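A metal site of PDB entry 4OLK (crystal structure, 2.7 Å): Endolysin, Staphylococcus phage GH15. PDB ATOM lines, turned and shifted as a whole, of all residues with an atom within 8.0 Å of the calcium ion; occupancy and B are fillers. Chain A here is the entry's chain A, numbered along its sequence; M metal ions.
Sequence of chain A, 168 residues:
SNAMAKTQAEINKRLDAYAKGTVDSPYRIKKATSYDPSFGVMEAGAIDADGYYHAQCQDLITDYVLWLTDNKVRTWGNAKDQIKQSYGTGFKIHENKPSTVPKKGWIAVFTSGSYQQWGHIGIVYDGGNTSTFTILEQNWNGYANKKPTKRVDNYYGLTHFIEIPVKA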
ATOM      1  N   TYR A  35      15.415   7.409 -15.078  1.00  0.00           N
ATOM      2  CA  TYR A  35      15.260   6.007 -15.418  1.00  0.00           C
ATOM      3  C   TYR A  35      13.887   5.770 -16.011  1.00  0.00           C
ATOM      4  O   TYR A  35      13.616   4.721 -16.561  1.00  0.00           O
ATOM      5  CB  TYR A  35      15.477   5.106 -14.200  1.00  0.00           C
ATOM      6  CG  TYR A  35      14.612   5.429 -13.009  1.00  0.00           C
ATOM      7  CD1 TYR A  35      13.331   4.908 -12.904  1.00  0.00           C
ATOM      8  CD2 TYR A  35      15.078   6.245 -11.990  1.00  0.00           C
ATOM      9  CE1 TYR A  35      12.547   5.201 -11.839  1.00  0.00           C
ATOM     10  CE2 TYR A  35      14.294   6.539 -10.925  1.00  0.00           C
ATOM     11  CZ  TYR A  35      13.038   6.019 -10.842  1.00  0.00           C
ATOM     12  OH  TYR A  35      12.260   6.322  -9.768  1.00  0.00           O
ATOM     13  N   PHE A  39       8.852  10.856 -16.960  1.00  0.00           N
ATOM     14  CA  PHE A  39       8.983  11.918 -15.984  1.00  0.00           C
ATOM     15  C   PHE A  39      10.213  12.734 -16.266  1.00  0.00           C
ATOM     16  O   PHE A  39      10.980  12.435 -17.170  1.00  0.00           O
ATOM     17  CB  PHE A  39       9.028  11.348 -14.568  1.00  0.00           C
ATOM     18  CG  PHE A  39       7.797  10.610 -14.192  1.00  0.00           C
ATOM     19  CD1 PHE A  39       6.686  11.279 -13.747  1.00  0.00           C
ATOM     20  CD2 PHE A  39       7.746   9.246 -14.290  1.00  0.00           C
ATOM     21  CE1 PHE A  39       5.558  10.605 -13.413  1.00  0.00           C
ATOM     22  CE2 PHE A  39       6.618   8.572 -13.957  1.00  0.00           C
ATOM     23  CZ  PHE A  39       5.518   9.247 -13.516  1.00  0.00           C
ATOM     24  N   MET A  42      15.426  13.869 -12.588  1.00  0.00           N
ATOM     25  CA  MET A  42      15.424  14.256 -11.188  1.00  0.00           C
ATOM     26  C   MET A  42      16.676  15.031 -10.835  1.00  0.00           C
ATOM     27  O   MET A  42      17.787  14.599 -11.144  1.00  0.00           O
ATOM     28  CB  MET A  42      15.296  13.037 -10.275  1.00  0.00           C
ATOM     29  CG  MET A  42      13.904  12.463 -10.179  1.00  0.00           C
ATOM     30  SD  MET A  42      13.824  11.100  -9.022  1.00  0.00           S
ATOM     31  CE  MET A  42      14.838   9.905  -9.843  1.00  0.00           C
ATOM     32  N   ILE A  47      13.922  13.355  -3.634  1.00  0.00           N
ATOM     33  CA  ILE A  47      13.750  12.162  -2.832  1.00  0.00           C
ATOM     34  C   ILE A  47      12.948  11.122  -3.592  1.00  0.00           C
ATOM     35  O   ILE A  47      11.785  11.323  -3.901  1.00  0.00           O
ATOM     36  CB  ILE A  47      13.061  12.486  -1.511  1.00  0.00           C
ATOM     37  CG1 ILE A  47      13.789  13.616  -0.799  1.00  0.00           C
ATOM     38  CG2 ILE A  47      13.016  11.274  -0.624  1.00  0.00           C
ATOM     39  CD1 ILE A  47      15.193  13.258  -0.434  1.00  0.00           C
ATOM     40  N   ASP A  48      13.601   9.998  -3.883  1.00  0.00           N
ATOM     41  CA  ASP A  48      12.979   8.872  -4.543  1.00  0.00           C
ATOM     42  C   ASP A  48      13.126   7.648  -3.655  1.00  0.00           C
ATOM     43  O   ASP A  48      14.155   6.988  -3.646  1.00  0.00           O
ATOM     44  CB  ASP A  48      13.616   8.654  -5.899  1.00  0.00           C
ATOM     45  CG  ASP A  48      12.957   7.563  -6.684  1.00  0.00           C
ATOM     46  OD1 ASP A  48      11.798   7.237  -6.401  1.00  0.00           O
ATOM     47  OD2 ASP A  48      13.602   7.037  -7.602  1.00  0.00           O
ATOM     48  N   ALA A  49      12.073   7.363  -2.902  1.00  0.00           N
ATOM     49  CA  ALA A  49      12.119   6.376  -1.822  1.00  0.00           C
ATOM     50  C   ALA A  49      11.815   4.967  -2.281  1.00  0.00           C
ATOM     51  O   ALA A  49      12.192   4.007  -1.634  1.00  0.00           O
ATOM     52  CB  ALA A  49      11.171   6.791  -0.696  1.00  0.00           C
ATOM     53  N   ASP A  50      11.107   4.825  -3.399  1.00  0.00           N
ATOM     54  CA  ASP A  50      10.761   3.499  -3.879  1.00  0.00           C
ATOM     55  C   ASP A  50      11.523   3.158  -5.157  1.00  0.00           C
ATOM     56  O   ASP A  50      11.736   1.997  -5.482  1.00  0.00           O
ATOM     57  CB  ASP A  50       9.249   3.357  -4.074  1.00  0.00           C
ATOM     58  CG  ASP A  50       8.664   4.422  -4.961  1.00  0.00           C
ATOM     59  OD1 ASP A  50       9.316   5.453  -5.199  1.00  0.00           O
ATOM     60  OD2 ASP A  50       7.520   4.244  -5.423  1.00  0.00           O
ATOM     61  N   GLY A  51      11.947   4.203  -5.863  1.00  0.00           N
ATOM     62  CA  GLY A  51      12.711   4.031  -7.076  1.00  0.00           C
ATOM     63  C   GLY A  51      11.826   3.974  -8.307  1.00  0.00           C
ATOM     64  O   GLY A  51      12.269   3.566  -9.390  1.00  0.00           O
ATOM     65  N   TYR A  52      10.576   4.415  -8.132  1.00  0.00           N
ATOM     66  CA  TYR A  52       9.560   4.363  -9.182  1.00  0.00           C
ATOM     67  C   TYR A  52       8.863   5.671  -9.322  1.00  0.00           C
ATOM     68  O   TYR A  52       8.496   6.322  -8.334  1.00  0.00           O
ATOM     69  CB  TYR A  52       8.576   3.215  -8.966  1.00  0.00           C
ATOM     70  CG  TYR A  52       9.333   1.986  -8.629  1.00  0.00           C
ATOM     71  CD1 TYR A  52       9.183   1.375  -7.381  1.00  0.00           C
ATOM     72  CD2 TYR A  52      10.226   1.452  -9.550  1.00  0.00           C
ATOM     73  CE1 TYR A  52       9.899   0.249  -7.074  1.00  0.00           C
ATOM     74  CE2 TYR A  52      10.978   0.285  -9.240  1.00  0.00           C
ATOM     75  CZ  TYR A  52      10.810  -0.311  -8.016  1.00  0.00           C
ATOM     76  OH  TYR A  52      11.550  -1.427  -7.762  1.00  0.00           O
ATOM     77  N   TYR A  53       8.680   6.031 -10.579  1.00  0.00           N
ATOM     78  CA  TYR A  53       7.977   7.234 -10.931  1.00  0.00           C
ATOM     79  C   TYR A  53       8.705   8.427 -10.380  1.00  0.00           C
ATOM     80  O   TYR A  53       8.082   9.430 -10.067  1.00  0.00           O
ATOM     81  CB  TYR A  53       6.565   7.183 -10.363  1.00  0.00           C
ATOM     82  CG  TYR A  53       5.866   5.884 -10.637  1.00  0.00           C
ATOM     83  CD1 TYR A  53       5.585   5.499 -11.931  1.00  0.00           C
ATOM     84  CD2 TYR A  53       5.476   5.047  -9.603  1.00  0.00           C
ATOM     85  CE1 TYR A  53       4.953   4.328 -12.194  1.00  0.00           C
ATOM     86  CE2 TYR A  53       4.830   3.859  -9.861  1.00  0.00           C
ATOM     87  CZ  TYR A  53       4.569   3.510 -11.162  1.00  0.00           C
ATOM     88  OH  TYR A  53       3.921   2.332 -11.429  1.00  0.00           O
ATOM     89  N   HIS A  54      10.016   8.298 -10.266  1.00  0.00           N
ATOM     90  CA  HIS A  54      10.858   9.409  -9.859  1.00  0.00           C
ATOM     91  C   HIS A  54      10.393  10.024  -8.544  1.00  0.00           C
ATOM     92  O   HIS A  54       9.822   9.340  -7.704  1.00  0.00           O
ATOM     93  CB  HIS A  54      10.897  10.443 -10.986  1.00  0.00           C
ATOM     94  CG  HIS A  54      11.771  10.057 -12.142  1.00  0.00           C
ATOM     95  ND1 HIS A  54      12.150  10.952 -13.112  1.00  0.00           N
ATOM     96  CD2 HIS A  54      12.342   8.879 -12.476  1.00  0.00           C
ATOM     97  CE1 HIS A  54      12.924  10.341 -13.995  1.00  0.00           C
ATOM     98  NE2 HIS A  54      13.056   9.089 -13.630  1.00  0.00           N
ATOM     99  N   ALA A  55      10.629  11.310  -8.369  1.00  0.00           N
ATOM    100  CA  ALA A  55      10.341  11.987  -7.107  1.00  0.00           C
ATOM    101  C   ALA A  55       8.887  12.380  -6.943  1.00  0.00           C
ATOM    102  O   ALA A  55       8.523  13.543  -7.109  1.00  0.00           O
ATOM    103  CB  ALA A  55      11.229  13.194  -6.957  1.00  0.00           C
ATOM    104  N   GLN A  56       8.060  11.406  -6.578  1.00  0.00           N
ATOM    105  CA  GLN A  56       6.659  11.643  -6.347  1.00  0.00           C
ATOM    106  C   GLN A  56       6.407  12.345  -5.024  1.00  0.00           C
ATOM    107  O   GLN A  56       7.311  12.557  -4.242  1.00  0.00           O
ATOM    108  CB  GLN A  56       5.906  10.322  -6.379  1.00  0.00           C
ATOM    109  CG  GLN A  56       5.979   9.598  -7.700  1.00  0.00           C
ATOM    110  CD  GLN A  56       5.019  10.157  -8.715  1.00  0.00           C
ATOM    111  OE1 GLN A  56       3.832  10.306  -8.433  1.00  0.00           O
ATOM    112  NE2 GLN A  56       5.515  10.467  -9.885  1.00  0.00           N
ATOM    113  N   CYS A  57       5.150  12.718  -4.795  1.00  0.00           N
ATOM    114  CA  CYS A  57       4.765  13.439  -3.597  1.00  0.00           C
ATOM    115  C   CYS A  57       4.966  12.617  -2.344  1.00  0.00           C
ATOM    116  O   CYS A  57       5.444  13.107  -1.331  1.00  0.00           O
ATOM    117  CB  CYS A  57       3.299  13.913  -3.706  1.00  0.00           C
ATOM    118  SG  CYS A  57       2.098  12.669  -4.179  1.00  0.00           S
ATOM    119  N   GLN A  58       4.586  11.346  -2.420  1.00  0.00           N
ATOM    120  CA  GLN A  58       4.627  10.468  -1.275  1.00  0.00           C
ATOM    121  C   GLN A  58       6.052  10.106  -0.887  1.00  0.00           C
ATOM    122  O   GLN A  58       6.324   9.904   0.285  1.00  0.00           O
ATOM    123  CB  GLN A  58       3.785   9.210  -1.537  1.00  0.00           C
ATOM    124  CG  GLN A  58       3.700   8.233  -0.375  1.00  0.00           C
ATOM    125  CD  GLN A  58       3.187   8.869   0.898  1.00  0.00           C
ATOM    126  OE1 GLN A  58       3.653   8.535   1.984  1.00  0.00           O
ATOM    127  NE2 GLN A  58       2.237   9.771   0.780  1.00  0.00           N
ATOM    128  N   ASP A  59       6.949  10.068  -1.855  1.00  0.00           N
ATOM    129  CA  ASP A  59       8.351   9.713  -1.620  1.00  0.00           C
ATOM    130  C   ASP A  59       9.013  10.511  -0.515  1.00  0.00           C
ATOM    131  O   ASP A  59       9.854  10.000   0.215  1.00  0.00           O
ATOM    132  CB  ASP A  59       9.158   9.858  -2.898  1.00  0.00           C
ATOM    133  CG  ASP A  59       9.112   8.633  -3.758  1.00  0.00           C
ATOM    134  OD1 ASP A  59       8.891   7.544  -3.202  1.00  0.00           O
ATOM    135  OD2 ASP A  59       9.291   8.748  -4.986  1.00  0.00           O
ATOM    136  N   LEU A  60       8.640  11.786  -0.407  1.00  0.00           N
ATOM    137  CA  LEU A  60       9.156  12.652   0.636  1.00  0.00           C
ATOM    138  C   LEU A  60       8.631  12.247   2.000  1.00  0.00           C
ATOM    139  O   LEU A  60       9.347  12.316   2.989  1.00  0.00           O
ATOM    140  CB  LEU A  60       8.783  14.100   0.337  1.00  0.00           C
ATOM    141  CG  LEU A  60       9.072  15.125   1.427  1.00  0.00           C
ATOM    142  CD1 LEU A  60      10.562  15.304   1.601  1.00  0.00           C
ATOM    143  CD2 LEU A  60       8.413  16.442   1.095  1.00  0.00           C
ATOM    144  N   GLN A 138       6.709  17.540  -2.846  1.00  0.00           N
ATOM    145  CA  GLN A 138       7.286  17.085  -4.102  1.00  0.00           C
ATOM    146  C   GLN A 138       6.156  16.829  -5.093  1.00  0.00           C
ATOM    147  O   GLN A 138       5.051  16.484  -4.704  1.00  0.00           O
ATOM    148  CB  GLN A 138       8.108  15.817  -3.918  1.00  0.00           C
ATOM    149  CG  GLN A 138       9.551  16.074  -3.530  1.00  0.00           C
ATOM    150  CD  GLN A 138      10.420  14.846  -3.661  1.00  0.00           C
ATOM    151  OE1 GLN A 138      11.640  14.951  -3.721  1.00  0.00           O
ATOM    152  NE2 GLN A 138       9.809  13.682  -3.714  1.00  0.00           N
ATOM    153  N   ALA A 144       7.501  15.097 -11.362  1.00  0.00           N
ATOM    154  CA  ALA A 144       8.329  14.277 -10.458  1.00  0.00           C
ATOM    155  C   ALA A 144       9.835  14.454 -10.566  1.00  0.00           C
ATOM    156  O   ALA A 144      10.581  13.499 -10.382  1.00  0.00           O
ATOM    157  CB  ALA A 144       7.945  12.816 -10.589  1.00  0.00           C
HETATM  158 CA    CA M   1       9.462   7.275  -6.708  1.00  0.00          CA
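N of His 54 is in hydrogen-bond range of OH of Tyr 35, at 3.0 Å.
The side-chain carboxylate (OD1) of Asp 48 lies close to the backbone NH (N) of Gly 51, at 3.1 Å.
The side-chain carboxylate of Asp 59 sits close to the backbone NH of Gln 56, at 3.3 Å.
The backbone carbonyl oxygen (O) of Tyr 53 lies within hydrogen-bond range of the side-chain amide nitrogen (NE2) of Gln 56 (2.8 Å).
N of Tyr 52 is in hydrogen-bond range of OH of Tyr 35, at 3.0 Å.
The backbone NH of Ala 49 lies within hydrogen-bond range of the side-chain carboxylate of Asp 59 (3.2 Å).
OD2 of Asp 48 is in hydrogen-bond range of OH of Tyr 35 (2.6 Å).
The calcium ion is bound by O of Tyr 52, OD2 of Asp 59, O of His 54, OD1 of Asp 48 and OD1 of Asp 50.
C of Tyr 53 touches the calcium ion, at 3.9 Å.
Of the 19 residues printed, 6 come within 4 Å of the calcium ion.
The nearest printed residue that does not touch the calcium ion is Gly 51 (4.04 Å).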
